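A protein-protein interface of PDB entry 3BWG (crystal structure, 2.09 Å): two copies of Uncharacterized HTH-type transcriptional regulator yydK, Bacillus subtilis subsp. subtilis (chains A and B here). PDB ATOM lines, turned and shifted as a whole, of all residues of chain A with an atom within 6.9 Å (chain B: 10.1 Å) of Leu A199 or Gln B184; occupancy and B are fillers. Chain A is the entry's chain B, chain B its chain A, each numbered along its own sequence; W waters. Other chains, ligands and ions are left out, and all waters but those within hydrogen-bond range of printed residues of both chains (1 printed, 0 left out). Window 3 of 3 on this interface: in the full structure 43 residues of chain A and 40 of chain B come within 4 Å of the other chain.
The backbone carbonyl oxygen of Gly A183 sits at hydrogen-bond distance from the backbone NH of Lys A201 (2.9 Å). The backbone NH (N) of Lys B201 lies within hydrogen-bond range of the backbone carbonyl oxygen (O) of Gly B183 (2.7 Å). The backbone carbonyl oxygen (O) of Gly A198 lies close to the side-chain amide oxygen (OE1) of Gln A184, 2.9 Å away. The backbone NH of Leu B185 is in hydrogen-bond range of the backbone carbonyl oxygen of Leu B199 (2.7 Å). O of Gly B198 lies within hydrogen-bond range of NE2 of Gln B184 (2.9 Å). O of Gln A184 sits at hydrogen-bond distance from NZ of Lys A201.
Gly A183 touches Pro B200 (O to CG, 3.4 Å). CD2 of Leu B199 touches OE1 of Gln A184, at 3.7 Å. CG of Gln A184 touches CG of Pro B200 (3.6 Å). Leu A199 touches Gln B184 (CD2 to NE2, 3.8 Å). Val B182 touches Pro A200 (CG1 to CB, 3.5 Å). Gly B183 touches Pro A200 (O to CG, 3.4 Å). Gln B184 touches Pro A200 (CG to CG, 3.6 Å). Pro A200 touches Pro B200 (CB to CB, 3.6 Å). Tyr A225 touches Val B182.
Of chain B, only Gln B184 comes within 4 Å of Leu A199. Of the printed residues of chain A, Gln B184 touches Leu A199 (3.8 Å) and Pro A200 (3.6 Å). No residue of chain B comes within 4 Å of Leu A185. No residue of chain B comes within 4 Å of Glu A196. No residue of chain B comes within 4 Å of Ala A197. Of chain B, only Val B182 (3.5 Å), Gly B183 (3.4 Å), Gln B184 (3.6 Å) and Pro B200 (3.6 Å) come within 4 Å of Pro A200. Of the printed residues of chain B, Gln A184 touches Leu B199 (3.7 Å) and Pro B200 (3.6 Å). Of the printed residues of chain B, Gly A183 touches Pro B200 (3.4 Å). Printed residues of chain A within 4 Å of Val B182: Pro A200 (3.5 Å) and Tyr A225 (3.7 Å). Tyr B225 touches none of the printed residues of chain A. Tyr B223 touches none of the printed residues of chain A. The nearest residue of chain B that does not touch Leu A199 is Pro B200 (5.4 Å). The nearest printed residue of chain A that does not touch Leu B199 is Pro A200 (5.2 Å).
Of the 14 printed residues of chain A, 5 touch a printed residue of chain B. Hydrophobic or aromatic side chains of chain A that line the printed part of chain B: Leu A199, Pro A200 and Tyr A225. Of the 23 printed residues of chain B, 5 touch a printed residue of chain A. Printed residues of chain B that touch a printed residue of chain A: Val B182, Gly B183, Gln B184, Leu B199 and Pro B200. Along chain B the printed residues that touch a printed residue of chain A span positions 182 to 200. Among the printed residues, no Asp or Glu carboxylate lies within 4 Å of a Lys or Arg side-chain nitrogen of the other chain.
Gly A183 touches Pro B200, and with the chains exchanged Pro A200 touches Gly B183. Gln A184 touches Leu B199, and with the chains exchanged Leu A199 touches Gln B184. Gln A184 touches Pro B200, and with the chains exchanged Pro A200 touches Gln B184. Pro B200 touches its own counterpart, Pro A200.
Water W1 lies within hydrogen-bond range of the backbone carbonyl oxygen (O) of Tyr A225 (2.9 Å) and the backbone NH (N) of Val B182 (2.9 Å).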
ATOM      1  N   GLY A 183      26.995  -8.114  30.712  1.00  0.00           N
ATOM      2  CA  GLY A 183      26.846  -6.966  29.857  1.00  0.00           C
ATOM      3  C   GLY A 183      27.966  -6.911  28.828  1.00  0.00           C
ATOM      4  O   GLY A 183      28.755  -7.862  28.702  1.00  0.00           O
ATOM      5  N   GLN A 184      27.988  -5.807  28.075  1.00  0.00           N
ATOM      6  CA  GLN A 184      29.042  -5.504  27.127  1.00  0.00           C
ATOM      7  C   GLN A 184      29.945  -4.438  27.735  1.00  0.00           C
ATOM      8  O   GLN A 184      29.464  -3.485  28.378  1.00  0.00           O
ATOM      9  CB  GLN A 184      28.457  -5.029  25.791  1.00  0.00           C
ATOM     10  CG  GLN A 184      27.779  -6.113  24.990  1.00  0.00           C
ATOM     11  CD  GLN A 184      27.228  -5.622  23.664  1.00  0.00           C
ATOM     12  OE1 GLN A 184      27.806  -5.881  22.619  1.00  0.00           O
ATOM     13  NE2 GLN A 184      26.117  -4.914  23.700  1.00  0.00           N
ATOM     14  N   LEU A 185      31.258  -4.606  27.559  1.00  0.00           N
ATOM     15  CA  LEU A 185      32.205  -3.576  27.956  1.00  0.00           C
ATOM     16  C   LEU A 185      31.991  -2.273  27.198  1.00  0.00           C
ATOM     17  O   LEU A 185      31.728  -2.270  26.004  1.00  0.00           O
ATOM     18  CB  LEU A 185      33.636  -4.030  27.727  1.00  0.00           C
ATOM     19  CG  LEU A 185      34.185  -5.192  28.529  1.00  0.00           C
ATOM     20  CD1 LEU A 185      35.383  -5.728  27.781  1.00  0.00           C
ATOM     21  CD2 LEU A 185      34.558  -4.747  29.939  1.00  0.00           C
ATOM     22  N   ASN A 186      32.109  -1.166  27.909  1.00  0.00           N
ATOM     23  CA  ASN A 186      32.072   0.127  27.285  1.00  0.00           C
ATOM     24  C   ASN A 186      33.502   0.574  27.058  1.00  0.00           C
ATOM     25  O   ASN A 186      34.433  -0.134  27.461  1.00  0.00           O
ATOM     26  CB  ASN A 186      31.274   1.105  28.151  1.00  0.00           C
ATOM     27  CG  ASN A 186      32.020   1.549  29.377  1.00  0.00           C
ATOM     28  OD1 ASN A 186      33.231   1.425  29.461  1.00  0.00           O
ATOM     29  ND2 ASN A 186      31.292   2.083  30.344  1.00  0.00           N
ATOM     30  N   ALA A 190      36.745  -1.170  28.542  1.00  0.00           N
ATOM     31  CA  ALA A 190      37.560  -1.877  27.560  1.00  0.00           C
ATOM     32  C   ALA A 190      39.014  -1.383  27.556  1.00  0.00           C
ATOM     33  O   ALA A 190      39.957  -2.181  27.473  1.00  0.00           O
ATOM     34  CB  ALA A 190      36.963  -1.750  26.156  1.00  0.00           C
ATOM     35  N   LEU A 195      40.820  -4.655  26.403  1.00  0.00           N
ATOM     36  CA  LEU A 195      39.971  -5.466  25.520  1.00  0.00           C
ATOM     37  C   LEU A 195      39.224  -4.509  24.594  1.00  0.00           C
ATOM     38  O   LEU A 195      39.434  -3.310  24.680  1.00  0.00           O
ATOM     39  CB  LEU A 195      38.974  -6.310  26.317  1.00  0.00           C
ATOM     40  CG  LEU A 195      39.574  -7.288  27.337  1.00  0.00           C
ATOM     41  CD1 LEU A 195      38.486  -7.824  28.263  1.00  0.00           C
ATOM     42  CD2 LEU A 195      40.329  -8.386  26.590  1.00  0.00           C
ATOM     43  N   GLU A 196      38.361  -5.024  23.726  1.00  0.00           N
ATOM     44  CA  GLU A 196      37.559  -4.173  22.827  1.00  0.00           C
ATOM     45  C   GLU A 196      36.186  -3.868  23.448  1.00  0.00           C
ATOM     46  O   GLU A 196      35.619  -4.715  24.131  1.00  0.00           O
ATOM     47  CB  GLU A 196      37.361  -4.873  21.496  1.00  0.00           C
ATOM     48  CG  GLU A 196      38.641  -5.460  20.928  1.00  0.00           C
ATOM     49  CD  GLU A 196      38.404  -6.584  19.929  1.00  0.00           C
ATOM     50  OE1 GLU A 196      39.223  -7.527  19.925  1.00  0.00           O
ATOM     51  OE2 GLU A 196      37.421  -6.532  19.142  1.00  0.00           O
ATOM     52  N   ALA A 197      35.654  -2.670  23.198  1.00  0.00           N
ATOM     53  CA  ALA A 197      34.306  -2.305  23.648  1.00  0.00           C
ATOM     54  C   ALA A 197      33.277  -3.229  22.999  1.00  0.00           C
ATOM     55  O   ALA A 197      33.449  -3.664  21.865  1.00  0.00           O
ATOM     56  CB  ALA A 197      33.997  -0.827  23.343  1.00  0.00           C
ATOM     57  N   GLY A 198      32.222  -3.556  23.732  1.00  0.00           N
ATOM     58  CA  GLY A 198      31.197  -4.433  23.189  1.00  0.00           C
ATOM     59  C   GLY A 198      31.421  -5.890  23.521  1.00  0.00           C
ATOM     60  O   GLY A 198      30.493  -6.690  23.472  1.00  0.00           O
ATOM     61  N   LEU A 199      32.651  -6.245  23.867  1.00  0.00           N
ATOM     62  CA  LEU A 199      32.942  -7.602  24.332  1.00  0.00           C
ATOM     63  C   LEU A 199      32.268  -7.830  25.691  1.00  0.00           C
ATOM     64  O   LEU A 199      31.891  -6.858  26.358  1.00  0.00           O
ATOM     65  CB  LEU A 199      34.464  -7.881  24.334  1.00  0.00           C
ATOM     66  CG  LEU A 199      35.103  -7.835  22.925  1.00  0.00           C
ATOM     67  CD1 LEU A 199      36.609  -7.937  23.017  1.00  0.00           C
ATOM     68  CD2 LEU A 199      34.565  -8.930  21.997  1.00  0.00           C
ATOM     69  N   PRO A 200      32.075  -9.112  26.084  1.00  0.00           N
ATOM     70  CA  PRO A 200      31.346  -9.486  27.305  1.00  0.00           C
ATOM     71  C   PRO A 200      32.079  -9.125  28.585  1.00  0.00           C
ATOM     72  O   PRO A 200      33.329  -9.139  28.634  1.00  0.00           O
ATOM     73  CB  PRO A 200      31.244 -11.009  27.212  1.00  0.00           C
ATOM     74  CG  PRO A 200      31.623 -11.356  25.821  1.00  0.00           C
ATOM     75  CD  PRO A 200      32.558 -10.302  25.363  1.00  0.00           C
ATOM     76  N   LYS A 201      31.310  -8.819  29.625  1.00  0.00           N
ATOM     77  CA  LYS A 201      31.873  -8.683  30.991  1.00  0.00           C
ATOM     78  C   LYS A 201      30.883  -9.213  32.024  1.00  0.00           C
ATOM     79  O   LYS A 201      29.657  -9.149  31.835  1.00  0.00           O
ATOM     80  CB  LYS A 201      32.182  -7.214  31.333  1.00  0.00           C
ATOM     81  CG  LYS A 201      30.959  -6.341  31.132  1.00  0.00           C
ATOM     82  CD  LYS A 201      30.987  -5.069  31.897  1.00  0.00           C
ATOM     83  CE  LYS A 201      29.599  -4.488  31.892  1.00  0.00           C
ATOM     84  NZ  LYS A 201      29.666  -3.034  31.785  1.00  0.00           N
ATOM     85  N   TYR A 225      36.675 -11.066  30.910  1.00  0.00           N
ATOM     86  CA  TYR A 225      36.112 -12.380  30.596  1.00  0.00           C
ATOM     87  C   TYR A 225      37.142 -13.424  30.138  1.00  0.00           C
ATOM     88  O   TYR A 225      36.899 -14.627  30.244  1.00  0.00           O
ATOM     89  CB  TYR A 225      34.956 -12.261  29.569  1.00  0.00           C
ATOM     90  CG  TYR A 225      35.388 -12.152  28.131  1.00  0.00           C
ATOM     91  CD1 TYR A 225      35.309 -13.244  27.284  1.00  0.00           C
ATOM     92  CD2 TYR A 225      35.880 -10.954  27.621  1.00  0.00           C
ATOM     93  CE1 TYR A 225      35.714 -13.162  25.939  1.00  0.00           C
ATOM     94  CE2 TYR A 225      36.308 -10.842  26.275  1.00  0.00           C
ATOM     95  CZ  TYR A 225      36.202 -11.951  25.452  1.00  0.00           C
ATOM     96  OH  TYR A 225      36.574 -11.861  24.149  1.00  0.00           O
ATOM     97  N   GLU A 226      38.295 -12.970  29.664  1.00  0.00           N
ATOM     98  CA  GLU A 226      39.336 -13.900  29.214  1.00  0.00           C
ATOM     99  C   GLU A 226      40.291 -14.331  30.312  1.00  0.00           C
ATOM    100  O   GLU A 226      41.137 -15.175  30.064  1.00  0.00           O
ATOM    101  CB  GLU A 226      40.222 -13.296  28.094  1.00  0.00           C
ATOM    102  CG  GLU A 226      39.541 -12.556  27.022  1.00  0.00           C
ATOM    103  CD  GLU A 226      40.492 -12.328  25.829  1.00  0.00           C
ATOM    104  OE1 GLU A 226      41.557 -11.665  25.991  1.00  0.00           O
ATOM    105  OE2 GLU A 226      40.172 -12.862  24.748  1.00  0.00           O
ATOM    106  N   HIS B 181      31.343 -18.788  33.965  1.00  0.00           N
ATOM    107  CA  HIS B 181      32.249 -18.309  32.966  1.00  0.00           C
ATOM    108  C   HIS B 181      31.455 -17.229  32.219  1.00  0.00           C
ATOM    109  O   HIS B 181      30.241 -17.258  32.228  1.00  0.00           O
ATOM    110  CB  HIS B 181      32.680 -19.438  32.004  1.00  0.00           C
ATOM    111  CG  HIS B 181      32.847 -20.787  32.656  1.00  0.00           C
ATOM    112  ND1 HIS B 181      31.775 -21.575  33.051  1.00  0.00           N
ATOM    113  CD2 HIS B 181      33.965 -21.488  32.980  1.00  0.00           C
ATOM    114  CE1 HIS B 181      32.224 -22.712  33.552  1.00  0.00           C
ATOM    115  NE2 HIS B 181      33.548 -22.677  33.534  1.00  0.00           N
ATOM    116  N   VAL B 182      32.147 -16.268  31.624  1.00  0.00           N
ATOM    117  CA  VAL B 182      31.528 -15.287  30.754  1.00  0.00           C
ATOM    118  C   VAL B 182      32.092 -15.459  29.352  1.00  0.00           C
ATOM    119  O   VAL B 182      33.309 -15.642  29.194  1.00  0.00           O
ATOM    120  CB  VAL B 182      31.753 -13.854  31.260  1.00  0.00           C
ATOM    121  CG1 VAL B 182      31.272 -12.832  30.240  1.00  0.00           C
ATOM    122  CG2 VAL B 182      30.959 -13.650  32.553  1.00  0.00           C
ATOM    123  N   GLY B 183      31.208 -15.434  28.349  1.00  0.00           N
ATOM    124  CA  GLY B 183      31.664 -15.419  26.960  1.00  0.00           C
ATOM    125  C   GLY B 183      30.673 -14.881  25.942  1.00  0.00           C
ATOM    126  O   GLY B 183      29.748 -14.141  26.280  1.00  0.00           O
ATOM    127  N   GLN B 184      30.898 -15.264  24.678  1.00  0.00           N
ATOM    128  CA  GLN B 184      30.087 -14.836  23.551  1.00  0.00           C
ATOM    129  C   GLN B 184      29.142 -15.957  23.161  1.00  0.00           C
ATOM    130  O   GLN B 184      29.536 -17.128  23.154  1.00  0.00           O
ATOM    131  CB  GLN B 184      30.986 -14.438  22.386  1.00  0.00           C
ATOM    132  CG  GLN B 184      31.768 -13.171  22.715  1.00  0.00           C
ATOM    133  CD  GLN B 184      32.570 -12.614  21.566  1.00  0.00           C
ATOM    134  OE1 GLN B 184      33.662 -13.098  21.258  1.00  0.00           O
ATOM    135  NE2 GLN B 184      32.073 -11.557  20.968  1.00  0.00           N
ATOM    136  N   LEU B 185      27.883 -15.613  22.871  1.00  0.00           N
ATOM    137  CA  LEU B 185      26.915 -16.605  22.369  1.00  0.00           C
ATOM    138  C   LEU B 185      27.381 -17.217  21.019  1.00  0.00           C
ATOM    139  O   LEU B 185      27.990 -16.540  20.215  1.00  0.00           O
ATOM    140  CB  LEU B 185      25.555 -15.943  22.178  1.00  0.00           C
ATOM    141  CG  LEU B 185      24.783 -15.553  23.429  1.00  0.00           C
ATOM    142  CD1 LEU B 185      23.736 -14.517  23.039  1.00  0.00           C
ATOM    143  CD2 LEU B 185      24.153 -16.801  24.047  1.00  0.00           C
ATOM    144  N   ASN B 186      27.143 -18.505  20.800  1.00  0.00           N
ATOM    145  CA  ASN B 186      27.376 -19.059  19.482  1.00  0.00           C
ATOM    146  C   ASN B 186      26.068 -19.138  18.714  1.00  0.00           C
ATOM    147  O   ASN B 186      25.032 -18.670  19.213  1.00  0.00           O
ATOM    148  CB  ASN B 186      28.154 -20.385  19.514  1.00  0.00           C
ATOM    149  CG  ASN B 186      27.348 -21.549  20.059  1.00  0.00           C
ATOM    150  OD1 ASN B 186      26.121 -21.520  20.139  1.00  0.00           O
ATOM    151  ND2 ASN B 186      28.048 -22.603  20.418  1.00  0.00           N
ATOM    152  N   GLU B 187      26.110 -19.705  17.505  1.00  0.00           N
ATOM    153  CA  GLU B 187      24.957 -19.692  16.615  1.00  0.00           C
ATOM    154  C   GLU B 187      23.751 -20.395  17.187  1.00  0.00           C
ATOM    155  O   GLU B 187      22.654 -19.848  17.153  1.00  0.00           O
ATOM    156  CB  GLU B 187      25.293 -20.300  15.244  1.00  0.00           C
ATOM    157  CG  GLU B 187      26.338 -19.527  14.453  1.00  0.00           C
ATOM    158  CD  GLU B 187      25.872 -18.132  14.013  1.00  0.00           C
ATOM    159  OE1 GLU B 187      24.635 -17.873  14.006  1.00  0.00           O
ATOM    160  OE2 GLU B 187      26.754 -17.297  13.680  1.00  0.00           O
ATOM    161  N   GLU B 188      23.937 -21.609  17.697  1.00  0.00           N
ATOM    162  CA  GLU B 188      22.783 -22.359  18.201  1.00  0.00           C
ATOM    163  C   GLU B 188      22.207 -21.801  19.515  1.00  0.00           C
ATOM    164  O   GLU B 188      20.992 -21.838  19.709  1.00  0.00           O
ATOM    165  CB  GLU B 188      23.067 -23.857  18.298  1.00  0.00           C
ATOM    166  CG  GLU B 188      24.004 -24.285  19.432  1.00  0.00           C
ATOM    167  CD  GLU B 188      24.341 -25.770  19.353  1.00  0.00           C
ATOM    168  OE1 GLU B 188      25.539 -26.090  19.137  1.00  0.00           O
ATOM    169  OE2 GLU B 188      23.408 -26.608  19.473  1.00  0.00           O
ATOM    170  N   GLU B 189      23.073 -21.274  20.389  1.00  0.00           N
ATOM    171  CA  GLU B 189      22.636 -20.635  21.644  1.00  0.00           C
ATOM    172  C   GLU B 189      21.856 -19.368  21.365  1.00  0.00           C
ATOM    173  O   GLU B 189      20.791 -19.132  21.948  1.00  0.00           O
ATOM    174  CB  GLU B 189      23.845 -20.241  22.492  1.00  0.00           C
ATOM    175  CG  GLU B 189      24.537 -21.382  23.099  1.00  0.00           C
ATOM    176  CD  GLU B 189      25.917 -21.026  23.510  1.00  0.00           C
ATOM    177  OE1 GLU B 189      26.358 -19.892  23.222  1.00  0.00           O
ATOM    178  OE2 GLU B 189      26.570 -21.899  24.115  1.00  0.00           O
ATOM    179  N   ALA B 190      22.437 -18.543  20.498  1.00  0.00           N
ATOM    180  CA  ALA B 190      21.833 -17.315  20.060  1.00  0.00           C
ATOM    181  C   ALA B 190      20.508 -17.578  19.343  1.00  0.00           C
ATOM    182  O   ALA B 190      19.547 -16.874  19.594  1.00  0.00           O
ATOM    183  CB  ALA B 190      22.789 -16.563  19.162  1.00  0.00           C
ATOM    184  N   LEU B 193      17.983 -18.724  21.991  1.00  0.00           N
ATOM    185  CA  LEU B 193      17.634 -17.626  22.910  1.00  0.00           C
ATOM    186  C   LEU B 193      17.001 -16.377  22.285  1.00  0.00           C
ATOM    187  O   LEU B 193      16.515 -15.516  23.008  1.00  0.00           O
ATOM    188  CB  LEU B 193      18.842 -17.229  23.775  1.00  0.00           C
ATOM    189  CG  LEU B 193      19.472 -18.266  24.717  1.00  0.00           C
ATOM    190  CD1 LEU B 193      20.670 -17.634  25.334  1.00  0.00           C
ATOM    191  CD2 LEU B 193      18.484 -18.706  25.782  1.00  0.00           C
ATOM    192  N   LEU B 195      18.597 -14.191  20.212  1.00  0.00           N
ATOM    193  CA  LEU B 195      19.634 -13.141  20.277  1.00  0.00           C
ATOM    194  C   LEU B 195      20.656 -13.341  19.153  1.00  0.00           C
ATOM    195  O   LEU B 195      20.625 -14.348  18.462  1.00  0.00           O
ATOM    196  CB  LEU B 195      20.390 -13.173  21.622  1.00  0.00           C
ATOM    197  CG  LEU B 195      19.639 -13.015  22.949  1.00  0.00           C
ATOM    198  CD1 LEU B 195      20.555 -13.410  24.130  1.00  0.00           C
ATOM    199  CD2 LEU B 195      19.108 -11.605  23.110  1.00  0.00           C
ATOM    200  N   GLU B 196      21.569 -12.392  18.989  1.00  0.00           N
ATOM    201  CA  GLU B 196      22.555 -12.467  17.925  1.00  0.00           C
ATOM    202  C   GLU B 196      23.807 -13.136  18.468  1.00  0.00           C
ATOM    203  O   GLU B 196      24.207 -12.857  19.602  1.00  0.00           O
ATOM    204  CB  GLU B 196      22.889 -11.068  17.434  1.00  0.00           C
ATOM    205  CG  GLU B 196      23.466 -11.014  16.023  1.00  0.00           C
ATOM    206  CD  GLU B 196      23.820  -9.583  15.577  1.00  0.00           C
ATOM    207  OE1 GLU B 196      23.093  -8.637  15.987  1.00  0.00           O
ATOM    208  OE2 GLU B 196      24.830  -9.408  14.841  1.00  0.00           O
ATOM    209  N   ALA B 197      24.404 -14.017  17.655  1.00  0.00           N
ATOM    210  CA  ALA B 197      25.714 -14.625  17.923  1.00  0.00           C
ATOM    211  C   ALA B 197      26.732 -13.551  18.237  1.00  0.00           C
ATOM    212  O   ALA B 197      26.727 -12.466  17.639  1.00  0.00           O
ATOM    213  CB  ALA B 197      26.190 -15.425  16.723  1.00  0.00           C
ATOM    214  N   GLY B 198      27.610 -13.844  19.192  1.00  0.00           N
ATOM    215  CA  GLY B 198      28.684 -12.917  19.505  1.00  0.00           C
ATOM    216  C   GLY B 198      28.328 -11.986  20.640  1.00  0.00           C
ATOM    217  O   GLY B 198      29.229 -11.418  21.270  1.00  0.00           O
ATOM    218  N   LEU B 199      27.032 -11.828  20.924  1.00  0.00           N
ATOM    219  CA  LEU B 199      26.613 -11.090  22.140  1.00  0.00           C
ATOM    220  C   LEU B 199      27.033 -11.821  23.462  1.00  0.00           C
ATOM    221  O   LEU B 199      27.344 -13.019  23.427  1.00  0.00           O
ATOM    222  CB  LEU B 199      25.106 -10.803  22.095  1.00  0.00           C
ATOM    223  CG  LEU B 199      24.693  -9.706  21.096  1.00  0.00           C
ATOM    224  CD1 LEU B 199      23.191  -9.611  20.940  1.00  0.00           C
ATOM    225  CD2 LEU B 199      25.250  -8.361  21.523  1.00  0.00           C
ATOM    226  N   PRO B 200      27.042 -11.114  24.619  1.00  0.00           N
ATOM    227  CA  PRO B 200      27.501 -11.764  25.869  1.00  0.00           C
ATOM    228  C   PRO B 200      26.586 -12.832  26.478  1.00  0.00           C
ATOM    229  O   PRO B 200      25.347 -12.800  26.278  1.00  0.00           O
ATOM    230  CB  PRO B 200      27.651 -10.605  26.860  1.00  0.00           C
ATOM    231  CG  PRO B 200      27.094  -9.443  26.242  1.00  0.00           C
ATOM    232  CD  PRO B 200      26.702  -9.697  24.825  1.00  0.00           C
ATOM    233  N   LYS B 201      27.195 -13.763  27.219  1.00  0.00           N
ATOM    234  CA  LYS B 201      26.426 -14.709  28.058  1.00  0.00           C
ATOM    235  C   LYS B 201      27.150 -15.063  29.347  1.00  0.00           C
ATOM    236  O   LYS B 201      28.381 -15.080  29.381  1.00  0.00           O
ATOM    237  CB  LYS B 201      26.148 -16.017  27.307  1.00  0.00           C
ATOM    238  CG  LYS B 201      27.440 -16.661  26.774  1.00  0.00           C
ATOM    239  CD  LYS B 201      27.343 -18.149  26.723  1.00  0.00           C
ATOM    240  CE  LYS B 201      28.609 -18.735  26.162  1.00  0.00           C
ATOM    241  NZ  LYS B 201      28.448 -20.227  26.044  1.00  0.00           N
ATOM    242  N   LEU B 202      26.388 -15.320  30.406  1.00  0.00           N
ATOM    243  CA  LEU B 202      26.874 -16.075  31.535  1.00  0.00           C
ATOM    244  C   LEU B 202      26.657 -17.541  31.197  1.00  0.00           C
ATOM    245  O   LEU B 202      25.542 -17.931  30.790  1.00  0.00           O
ATOM    246  CB  LEU B 202      26.086 -15.750  32.818  1.00  0.00           C
ATOM    247  CG  LEU B 202      26.620 -16.361  34.110  1.00  0.00           C
ATOM    248  CD1 LEU B 202      27.998 -15.839  34.448  1.00  0.00           C
ATOM    249  CD2 LEU B 202      25.620 -16.087  35.271  1.00  0.00           C
ATOM    250  N   TYR B 203      27.723 -18.331  31.379  1.00  0.00           N
ATOM    251  CA  TYR B 203      27.735 -19.753  31.140  1.00  0.00           C
ATOM    252  C   TYR B 203      28.110 -20.501  32.435  1.00  0.00           C
ATOM    253  O   TYR B 203      29.183 -20.315  32.994  1.00  0.00           O
ATOM    254  CB  TYR B 203      28.698 -20.085  29.975  1.00  0.00           C
ATOM    255  CG  TYR B 203      28.852 -21.577  29.761  1.00  0.00           C
ATOM    256  CD1 TYR B 203      27.788 -22.331  29.236  1.00  0.00           C
ATOM    257  CD2 TYR B 203      30.037 -22.237  30.097  1.00  0.00           C
ATOM    258  CE1 TYR B 203      27.890 -23.722  29.052  1.00  0.00           C
ATOM    259  CE2 TYR B 203      30.171 -23.595  29.906  1.00  0.00           C
ATOM    260  CZ  TYR B 203      29.085 -24.342  29.372  1.00  0.00           C
ATOM    261  OH  TYR B 203      29.205 -25.699  29.169  1.00  0.00           O
ATOM    262  N   SER B 222      23.447 -21.626  29.520  1.00  0.00           N
ATOM    263  CA  SER B 222      23.747 -20.321  28.967  1.00  0.00           C
ATOM    264  C   SER B 222      22.540 -19.429  29.141  1.00  0.00           C
ATOM    265  O   SER B 222      21.481 -19.737  28.631  1.00  0.00           O
ATOM    266  CB  SER B 222      24.079 -20.411  27.445  1.00  0.00           C
ATOM    267  OG  SER B 222      25.342 -21.033  27.246  1.00  0.00           O
ATOM    268  N   TYR B 223      22.726 -18.315  29.833  1.00  0.00           N
ATOM    269  CA  TYR B 223      21.636 -17.421  30.199  1.00  0.00           C
ATOM    270  C   TYR B 223      21.488 -16.284  29.212  1.00  0.00           C
ATOM    271  O   TYR B 223      22.474 -15.846  28.595  1.00  0.00           O
ATOM    272  CB  TYR B 223      21.866 -16.854  31.607  1.00  0.00           C
ATOM    273  CG  TYR B 223      21.568 -17.857  32.696  1.00  0.00           C
ATOM    274  CD1 TYR B 223      20.260 -18.065  33.122  1.00  0.00           C
ATOM    275  CD2 TYR B 223      22.597 -18.608  33.277  1.00  0.00           C
ATOM    276  CE1 TYR B 223      19.959 -19.001  34.115  1.00  0.00           C
ATOM    277  CE2 TYR B 223      22.322 -19.547  34.254  1.00  0.00           C
ATOM    278  CZ  TYR B 223      21.013 -19.730  34.688  1.00  0.00           C
ATOM    279  OH  TYR B 223      20.746 -20.677  35.659  1.00  0.00           O
ATOM    280  N   TYR B 225      21.373 -12.676  28.668  1.00  0.00           N
ATOM    281  CA  TYR B 225      21.935 -11.559  29.466  1.00  0.00           C
ATOM    282  C   TYR B 225      20.959 -10.385  29.665  1.00  0.00           C
ATOM    283  O   TYR B 225      21.162  -9.535  30.534  1.00  0.00           O
ATOM    284  CB  TYR B 225      23.243 -11.065  28.848  1.00  0.00           C
ATOM    285  CG  TYR B 225      23.078 -10.111  27.646  1.00  0.00           C
ATOM    286  CD1 TYR B 225      23.377  -8.758  27.779  1.00  0.00           C
ATOM    287  CD2 TYR B 225      22.630 -10.570  26.394  1.00  0.00           C
ATOM    288  CE1 TYR B 225      23.257  -7.880  26.702  1.00  0.00           C
ATOM    289  CE2 TYR B 225      22.492  -9.702  25.314  1.00  0.00           C
ATOM    290  CZ  TYR B 225      22.808  -8.351  25.480  1.00  0.00           C
ATOM    291  OH  TYR B 225      22.711  -7.459  24.435  1.00  0.00           O
HETATM  292  O   HOH W   1      34.932 -15.590  32.139  1.00  0.00           O
